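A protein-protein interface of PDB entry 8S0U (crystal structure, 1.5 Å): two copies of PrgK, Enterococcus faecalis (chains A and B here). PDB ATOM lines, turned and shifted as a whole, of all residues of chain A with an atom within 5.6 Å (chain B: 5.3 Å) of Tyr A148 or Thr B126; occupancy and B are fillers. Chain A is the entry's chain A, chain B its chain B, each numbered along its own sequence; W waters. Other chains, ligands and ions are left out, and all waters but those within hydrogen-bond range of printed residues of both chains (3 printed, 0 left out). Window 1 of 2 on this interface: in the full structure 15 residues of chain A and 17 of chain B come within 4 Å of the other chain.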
ATOM      1  N   THR A  24      -8.149  -9.060  34.628  1.00  0.00           N
ATOM      2  CA  THR A  24      -8.981  -9.239  33.448  1.00  0.00           C
ATOM      3  C   THR A  24      -8.312 -10.166  32.449  1.00  0.00           C
ATOM      4  O   THR A  24      -8.964 -11.018  31.871  1.00  0.00           O
ATOM      5  CB  THR A  24      -9.262  -7.877  32.853  1.00  0.00           C
ATOM      6  OG1 THR A  24      -9.982  -7.086  33.806  1.00  0.00           O
ATOM      7  CG2 THR A  24     -10.112  -7.978  31.576  1.00  0.00           C
ATOM      8  N   THR A  27      -9.000 -13.610  33.463  1.00  0.00           N
ATOM      9  CA  THR A  27     -10.392 -14.023  33.178  1.00  0.00           C
ATOM     10  C   THR A  27     -10.593 -14.273  31.679  1.00  0.00           C
ATOM     11  O   THR A  27     -11.398 -15.133  31.307  1.00  0.00           O
ATOM     12  CB  THR A  27     -11.482 -13.039  33.602  1.00  0.00           C
ATOM     13  OG1 THR A  27     -11.405 -11.817  32.841  1.00  0.00           O
ATOM     14  CG2 THR A  27     -11.400 -12.710  35.120  1.00  0.00           C
ATOM     15  N   LYS A  28      -9.803 -13.583  30.827  1.00  0.00           N
ATOM     16  CA  LYS A  28      -9.876 -13.855  29.385  1.00  0.00           C
ATOM     17  C   LYS A  28      -9.458 -15.274  29.091  1.00  0.00           C
ATOM     18  O   LYS A  28     -10.140 -15.995  28.341  1.00  0.00           O
ATOM     19  CB  LYS A  28      -9.002 -12.866  28.630  1.00  0.00           C
ATOM     20  CG  LYS A  28      -9.211 -12.915  27.097  1.00  0.00           C
ATOM     21  CD  LYS A  28      -8.218 -11.986  26.369  1.00  0.00           C
ATOM     22  CE  LYS A  28      -6.770 -12.401  26.544  1.00  0.00           C
ATOM     23  NZ  LYS A  28      -5.850 -11.731  25.518  1.00  0.00           N
ATOM     24  N   ALA A  31     -12.124 -17.677  30.248  1.00  0.00           N
ATOM     25  CA  ALA A  31     -13.322 -17.636  29.418  1.00  0.00           C
ATOM     26  C   ALA A  31     -13.075 -18.268  28.063  1.00  0.00           C
ATOM     27  O   ALA A  31     -13.943 -18.979  27.531  1.00  0.00           O
ATOM     28  CB  ALA A  31     -13.768 -16.200  29.239  1.00  0.00           C
ATOM     29  N   GLN A  32     -11.862 -18.106  27.526  1.00  0.00           N
ATOM     30  CA  GLN A  32     -11.573 -18.629  26.199  1.00  0.00           C
ATOM     31  C   GLN A  32     -11.509 -20.144  26.199  1.00  0.00           C
ATOM     32  O   GLN A  32     -11.761 -20.774  25.169  1.00  0.00           O
ATOM     33  CB  GLN A  32     -10.258 -18.054  25.704  1.00  0.00           C
ATOM     34  CG  GLN A  32     -10.324 -16.649  25.144  1.00  0.00           C
ATOM     35  CD  GLN A  32      -8.998 -16.031  24.831  1.00  0.00           C
ATOM     36  OE1 GLN A  32      -7.965 -16.499  25.301  1.00  0.00           O
ATOM     37  NE2 GLN A  32      -9.001 -15.002  23.995  1.00  0.00           N
ATOM     38  N   ARG A 145     -18.485 -12.421  38.967  1.00  0.00           N
ATOM     39  CA  ARG A 145     -17.256 -11.683  39.175  1.00  0.00           C
ATOM     40  C   ARG A 145     -16.971 -10.777  37.979  1.00  0.00           C
ATOM     41  O   ARG A 145     -17.590 -10.851  36.921  1.00  0.00           O
ATOM     42  CB  ARG A 145     -16.086 -12.635  39.397  1.00  0.00           C
ATOM     43  CG  ARG A 145     -15.693 -13.427  38.123  1.00  0.00           C
ATOM     44  CD  ARG A 145     -14.616 -14.408  38.401  1.00  0.00           C
ATOM     45  NE  ARG A 145     -14.100 -15.020  37.175  1.00  0.00           N
ATOM     46  CZ  ARG A 145     -13.035 -15.795  37.123  1.00  0.00           C
ATOM     47  NH1 ARG A 145     -12.404 -16.168  38.228  1.00  0.00           N
ATOM     48  NH2 ARG A 145     -12.661 -16.263  35.948  1.00  0.00           N
ATOM     49  N   TYR A 146     -16.003  -9.893  38.192  1.00  0.00           N
ATOM     50  CA  TYR A 146     -15.566  -8.969  37.151  1.00  0.00           C
ATOM     51  C   TYR A 146     -14.790  -9.684  36.054  1.00  0.00           C
ATOM     52  O   TYR A 146     -13.994 -10.591  36.310  1.00  0.00           O
ATOM     53  CB  TYR A 146     -14.643  -7.925  37.827  1.00  0.00           C
ATOM     54  CG  TYR A 146     -14.188  -6.806  36.946  1.00  0.00           C
ATOM     55  CD1 TYR A 146     -13.120  -6.968  36.106  1.00  0.00           C
ATOM     56  CD2 TYR A 146     -14.856  -5.606  36.953  1.00  0.00           C
ATOM     57  CE1 TYR A 146     -12.725  -5.945  35.240  1.00  0.00           C
ATOM     58  CE2 TYR A 146     -14.488  -4.568  36.099  1.00  0.00           C
ATOM     59  CZ  TYR A 146     -13.419  -4.764  35.281  1.00  0.00           C
ATOM     60  OH  TYR A 146     -12.994  -3.751  34.407  1.00  0.00           O
ATOM     61  N   GLY A 147     -14.970  -9.218  34.807  1.00  0.00           N
ATOM     62  CA  GLY A 147     -14.127  -9.626  33.714  1.00  0.00           C
ATOM     63  C   GLY A 147     -14.844 -10.458  32.665  1.00  0.00           C
ATOM     64  O   GLY A 147     -16.065 -10.427  32.532  1.00  0.00           O
ATOM     65  N   TYR A 148     -14.053 -11.240  31.948  1.00  0.00           N
ATOM     66  CA  TYR A 148     -14.607 -12.033  30.862  1.00  0.00           C
ATOM     67  C   TYR A 148     -15.314 -13.290  31.350  1.00  0.00           C
ATOM     68  O   TYR A 148     -14.905 -13.920  32.337  1.00  0.00           O
ATOM     69  CB  TYR A 148     -13.498 -12.432  29.892  1.00  0.00           C
ATOM     70  CG  TYR A 148     -12.971 -11.295  29.042  1.00  0.00           C
ATOM     71  CD1 TYR A 148     -13.683 -10.898  27.926  1.00  0.00           C
ATOM     72  CD2 TYR A 148     -11.781 -10.635  29.333  1.00  0.00           C
ATOM     73  CE1 TYR A 148     -13.237  -9.878  27.126  1.00  0.00           C
ATOM     74  CE2 TYR A 148     -11.324  -9.580  28.550  1.00  0.00           C
ATOM     75  CZ  TYR A 148     -12.076  -9.232  27.427  1.00  0.00           C
ATOM     76  OH  TYR A 148     -11.600  -8.180  26.632  1.00  0.00           O
ATOM     77  N   ASP A 149     -16.294 -13.744  30.582  1.00  0.00           N
ATOM     78  CA  ASP A 149     -16.864 -15.071  30.762  1.00  0.00           C
ATOM     79  C   ASP A 149     -17.515 -15.446  29.451  1.00  0.00           C
ATOM     80  O   ASP A 149     -17.589 -14.617  28.535  1.00  0.00           O
ATOM     81  CB  ASP A 149     -17.917 -15.082  31.872  1.00  0.00           C
ATOM     82  CG  ASP A 149     -18.208 -16.491  32.432  1.00  0.00           C
ATOM     83  OD1 ASP A 149     -17.665 -17.547  31.960  1.00  0.00           O
ATOM     84  OD2 ASP A 149     -19.077 -16.555  33.344  1.00  0.00           O
ATOM     85  N   LYS A 150     -18.026 -16.656  29.392  1.00  0.00           N
ATOM     86  CA  LYS A 150     -18.888 -17.083  28.292  1.00  0.00           C
ATOM     87  C   LYS A 150     -20.338 -16.920  28.735  1.00  0.00           C
ATOM     88  O   LYS A 150     -20.713 -17.389  29.816  1.00  0.00           O
ATOM     89  CB  LYS A 150     -18.660 -18.540  27.888  1.00  0.00           C
ATOM     90  CG  LYS A 150     -17.290 -18.807  27.221  1.00  0.00           C
ATOM     91  CD  LYS A 150     -17.195 -18.151  25.808  1.00  0.00           C
ATOM     92  CE  LYS A 150     -16.671 -19.119  24.791  1.00  0.00           C
ATOM     93  NZ  LYS A 150     -15.305 -19.592  25.097  1.00  0.00           N
ATOM     94  N   LEU A 155     -18.223 -14.887  24.205  1.00  0.00           N
ATOM     95  CA  LEU A 155     -17.333 -14.128  25.078  1.00  0.00           C
ATOM     96  C   LEU A 155     -17.889 -12.742  25.368  1.00  0.00           C
ATOM     97  O   LEU A 155     -18.284 -12.012  24.458  1.00  0.00           O
ATOM     98  CB  LEU A 155     -15.981 -14.004  24.406  1.00  0.00           C
ATOM     99  CG  LEU A 155     -14.860 -13.393  25.188  1.00  0.00           C
ATOM    100  CD1 LEU A 155     -14.388 -14.338  26.344  1.00  0.00           C
ATOM    101  CD2 LEU A 155     -13.716 -13.043  24.259  1.00  0.00           C
ATOM    102  N   THR A 156     -17.896 -12.351  26.647  1.00  0.00           N
ATOM    103  CA  THR A 156     -18.520 -11.141  27.107  1.00  0.00           C
ATOM    104  C   THR A 156     -17.676 -10.585  28.250  1.00  0.00           C
ATOM    105  O   THR A 156     -17.154 -11.358  29.050  1.00  0.00           O
ATOM    106  CB  THR A 156     -19.924 -11.488  27.626  1.00  0.00           C
ATOM    107  OG1 THR A 156     -20.625 -12.187  26.561  1.00  0.00           O
ATOM    108  CG2 THR A 156     -20.650 -10.281  28.011  1.00  0.00           C
ATOM    109  N   LEU A 157     -17.551  -9.279  28.350  1.00  0.00           N
ATOM    110  CA  LEU A 157     -16.799  -8.634  29.417  1.00  0.00           C
ATOM    111  C   LEU A 157     -17.764  -7.971  30.381  1.00  0.00           C
ATOM    112  O   LEU A 157     -18.615  -7.182  29.990  1.00  0.00           O
ATOM    113  CB  LEU A 157     -15.878  -7.575  28.810  1.00  0.00           C
ATOM    114  CG  LEU A 157     -15.074  -6.687  29.755  1.00  0.00           C
ATOM    115  CD1 LEU A 157     -14.100  -7.417  30.592  1.00  0.00           C
ATOM    116  CD2 LEU A 157     -14.321  -5.670  28.944  1.00  0.00           C
ATOM    117  N   TYR A 158     -17.656  -8.299  31.647  1.00  0.00           N
ATOM    118  CA  TYR A 158     -18.551  -7.760  32.663  1.00  0.00           C
ATOM    119  C   TYR A 158     -17.760  -6.764  33.485  1.00  0.00           C
ATOM    120  O   TYR A 158     -16.851  -7.150  34.232  1.00  0.00           O
ATOM    121  CB  TYR A 158     -19.172  -8.846  33.526  1.00  0.00           C
ATOM    122  CG  TYR A 158     -20.393  -8.410  34.268  1.00  0.00           C
ATOM    123  CD1 TYR A 158     -21.553  -8.080  33.596  1.00  0.00           C
ATOM    124  CD2 TYR A 158     -20.439  -8.312  35.659  1.00  0.00           C
ATOM    125  CE1 TYR A 158     -22.689  -7.728  34.235  1.00  0.00           C
ATOM    126  CE2 TYR A 158     -21.599  -7.952  36.312  1.00  0.00           C
ATOM    127  CZ  TYR A 158     -22.736  -7.644  35.594  1.00  0.00           C
ATOM    128  OH  TYR A 158     -23.901  -7.253  36.186  1.00  0.00           O
ATOM    129  N   PRO B  10     -17.247  -7.874  23.009  1.00  0.00           N
ATOM    130  CA  PRO B  10     -15.918  -7.564  22.461  1.00  0.00           C
ATOM    131  C   PRO B  10     -16.019  -6.773  21.162  1.00  0.00           C
ATOM    132  O   PRO B  10     -17.085  -6.679  20.531  1.00  0.00           O
ATOM    133  CB  PRO B  10     -15.301  -8.932  22.197  1.00  0.00           C
ATOM    134  CG  PRO B  10     -16.078  -9.881  23.114  1.00  0.00           C
ATOM    135  CD  PRO B  10     -17.478  -9.321  23.087  1.00  0.00           C
ATOM    136  N   ALA B  11     -14.873  -6.220  20.762  1.00  0.00           N
ATOM    137  CA  ALA B  11     -14.806  -5.530  19.486  1.00  0.00           C
ATOM    138  C   ALA B  11     -14.961  -6.490  18.339  1.00  0.00           C
ATOM    139  O   ALA B  11     -15.590  -6.146  17.328  1.00  0.00           O
ATOM    140  CB  ALA B  11     -13.499  -4.792  19.354  1.00  0.00           C
ATOM    141  N   ILE B  12     -14.428  -7.691  18.451  1.00  0.00           N
ATOM    142  CA  ILE B  12     -14.589  -8.732  17.449  1.00  0.00           C
ATOM    143  C   ILE B  12     -15.393  -9.857  18.064  1.00  0.00           C
ATOM    144  O   ILE B  12     -14.991 -10.415  19.096  1.00  0.00           O
ATOM    145  CB  ILE B  12     -13.230  -9.236  16.935  1.00  0.00           C
ATOM    146  CG1 ILE B  12     -12.493  -8.136  16.216  1.00  0.00           C
ATOM    147  CG2 ILE B  12     -13.409 -10.419  16.019  1.00  0.00           C
ATOM    148  CD1 ILE B  12     -13.160  -7.596  14.972  1.00  0.00           C
ATOM    149  N   LEU B 122      -9.754  -3.098  23.003  1.00  0.00           N
ATOM    150  CA  LEU B 122      -9.734  -4.552  22.848  1.00  0.00           C
ATOM    151  C   LEU B 122      -9.142  -5.040  21.540  1.00  0.00           C
ATOM    152  O   LEU B 122      -8.513  -6.103  21.524  1.00  0.00           O
ATOM    153  CB  LEU B 122     -11.130  -5.146  22.988  1.00  0.00           C
ATOM    154  CG  LEU B 122     -11.890  -4.764  24.288  1.00  0.00           C
ATOM    155  CD1 LEU B 122     -13.159  -5.619  24.421  1.00  0.00           C
ATOM    156  CD2 LEU B 122     -11.073  -4.836  25.566  1.00  0.00           C
ATOM    157  N   GLY B 123      -9.331  -4.303  20.444  1.00  0.00           N
ATOM    158  CA  GLY B 123      -8.870  -4.770  19.161  1.00  0.00           C
ATOM    159  C   GLY B 123      -9.211  -6.217  18.850  1.00  0.00           C
ATOM    160  O   GLY B 123     -10.322  -6.690  19.052  1.00  0.00           O
ATOM    161  N   TYR B 124      -8.221  -6.930  18.330  1.00  0.00           N
ATOM    162  CA  TYR B 124      -8.329  -8.351  18.056  1.00  0.00           C
ATOM    163  C   TYR B 124      -7.798  -9.189  19.203  1.00  0.00           C
ATOM    164  O   TYR B 124      -7.608 -10.400  19.045  1.00  0.00           O
ATOM    165  CB  TYR B 124      -7.522  -8.680  16.805  1.00  0.00           C
ATOM    166  CG  TYR B 124      -7.986  -8.027  15.503  1.00  0.00           C
ATOM    167  CD1 TYR B 124      -9.095  -8.498  14.822  1.00  0.00           C
ATOM    168  CD2 TYR B 124      -7.274  -6.999  14.934  1.00  0.00           C
ATOM    169  CE1 TYR B 124      -9.479  -7.969  13.605  1.00  0.00           C
ATOM    170  CE2 TYR B 124      -7.712  -6.448  13.688  1.00  0.00           C
ATOM    171  CZ  TYR B 124      -8.812  -6.917  13.097  1.00  0.00           C
ATOM    172  OH  TYR B 124      -9.257  -6.426  11.871  1.00  0.00           O
ATOM    173  N   GLN B 125      -7.503  -8.564  20.348  1.00  0.00           N
ATOM    174  CA  GLN B 125      -6.812  -9.284  21.427  1.00  0.00           C
ATOM    175  C   GLN B 125      -7.713 -10.258  22.142  1.00  0.00           C
ATOM    176  O   GLN B 125      -7.221 -10.955  23.018  1.00  0.00           O
ATOM    177  CB  GLN B 125      -6.170  -8.270  22.357  1.00  0.00           C
ATOM    178  CG  GLN B 125      -5.031  -7.505  21.720  1.00  0.00           C
ATOM    179  CD  GLN B 125      -3.750  -8.310  21.718  1.00  0.00           C
ATOM    180  OE1 GLN B 125      -3.325  -8.785  20.689  1.00  0.00           O
ATOM    181  NE2 GLN B 125      -3.119  -8.454  22.888  1.00  0.00           N
ATOM    182  N   THR B 126      -8.986 -10.340  21.839  1.00  0.00           N
ATOM    183  CA  THR B 126      -9.833 -11.389  22.356  1.00  0.00           C
ATOM    184  C   THR B 126      -9.810 -12.680  21.530  1.00  0.00           C
ATOM    185  O   THR B 126     -10.424 -13.689  21.925  1.00  0.00           O
ATOM    186  CB  THR B 126     -11.272 -10.884  22.482  1.00  0.00           C
ATOM    187  OG1 THR B 126     -11.715 -10.353  21.217  1.00  0.00           O
ATOM    188  CG2 THR B 126     -11.346  -9.746  23.521  1.00  0.00           C
ATOM    189  N   LEU B 127      -9.080 -12.720  20.401  1.00  0.00           N
ATOM    190  CA  LEU B 127      -8.933 -13.958  19.663  1.00  0.00           C
ATOM    191  C   LEU B 127      -8.031 -14.932  20.429  1.00  0.00           C
ATOM    192  O   LEU B 127      -7.211 -14.526  21.241  1.00  0.00           O
ATOM    193  CB  LEU B 127      -8.289 -13.663  18.291  1.00  0.00           C
ATOM    194  CG  LEU B 127      -9.157 -12.818  17.324  1.00  0.00           C
ATOM    195  CD1 LEU B 127      -8.373 -12.551  16.034  1.00  0.00           C
ATOM    196  CD2 LEU B 127     -10.498 -13.482  17.013  1.00  0.00           C
ATOM    197  N   ASP B 128      -8.213 -16.220  20.177  1.00  0.00           N
ATOM    198  CA  ASP B 128      -7.407 -17.250  20.839  1.00  0.00           C
ATOM    199  C   ASP B 128      -6.012 -17.350  20.216  1.00  0.00           C
ATOM    200  O   ASP B 128      -5.814 -17.109  19.002  1.00  0.00           O
ATOM    201  CB  ASP B 128      -8.061 -18.638  20.705  1.00  0.00           C
ATOM    202  CG  ASP B 128      -9.437 -18.756  21.401  1.00  0.00           C
ATOM    203  OD1 ASP B 128      -9.756 -17.945  22.308  1.00  0.00           O
ATOM    204  OD2 ASP B 128     -10.177 -19.726  21.101  1.00  0.00           O
HETATM  205  O   HOH W   1      -3.112 -10.240  25.255  1.00  0.00           O
HETATM  206  O   HOH W   2      -6.050 -14.800  23.776  1.00  0.00           O
HETATM  207  O   HOH W   3     -11.949 -20.534  22.730  1.00  0.00           O
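The side-chain amide nitrogen (NE2) of Gln A32 sits at hydrogen-bond distance from the backbone carbonyl oxygen (O) of Leu B127, 3.3 Å away.
The side-chain amino group (NZ) of Lys A28 is in hydrogen-bond range of the backbone carbonyl oxygen (O) of Gln B125, 3.0 Å away.
The side-chain amide nitrogen (NE2) of Gln A32 sits at hydrogen-bond distance from the backbone carbonyl oxygen (O) of Thr B126.
OD1 of Asp B128 lies close to NE2 of Gln A32, 3.5 Å away.
The side-chain hydroxyl of Thr A27 is in hydrogen-bond range of the backbone NH of Tyr A148, 2.9 Å away.
Among the printed residues, merely in contact across the chains: Tyr A148 with Leu B122, Tyr A148 with Thr B126, Leu A155 with Pro B10 and Leu A155 with Thr B126.
Of the printed residues of chain B, Tyr A148 touches Leu B122 (3.5 Å) and Thr B126 (3.5 Å).
Lys A150 touches none of the printed residues of chain B.
Of the printed residues of chain B, Leu A155 touches Pro B10 and Thr B126.
Ile B12 touches none of the printed residues of chain A.
Of the printed residues of chain A, Gln B125 touches Lys A28 (3.0 Å).
Thr B126 touches three residues of chain A.
Of the printed residues of chain A, Leu B127 touches Gln A32.
Of the printed residues of chain A, Asp B128 touches Gln A32 (3.2 Å).
The nearest residue of chain B that does not touch Tyr A148 is Pro B10 (4.9 Å).
The nearest printed residue of chain A that does not touch Asp B128 is Lys A28 (6.4 Å).
Printed residues of chain B that touch a printed residue of chain A: Pro B10, Leu B122, Gln B125, Thr B126, Leu B127 and Asp B128.
Of the 15 printed residues of chain A, 4 touch a printed residue of chain B.
Printed residues of chain A that touch a printed residue of chain B: Lys A28, Gln A32, Tyr A148 and Leu A155.
No position is printed for both chains.
Of the 8 pairs that touch across the chains among the printed residues, none has its exchanged pair printed and touching as well.
Water W3 bridges O of Gln A32 (2.5 Å) and OD2 of Asp B128 (2.5 Å).
Water W2 lies within hydrogen-bond range of the backbone carbonyl oxygen (O) of Leu B127 (2.8 Å) and the side-chain amide nitrogen (NE2) of Gln A32 (3.0 Å).
Water W1 bridges the side-chain amide nitrogen (NE2) of Gln B125 (3.0 Å) and the side-chain amino group (NZ) of Lys A28 (3.1 Å).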
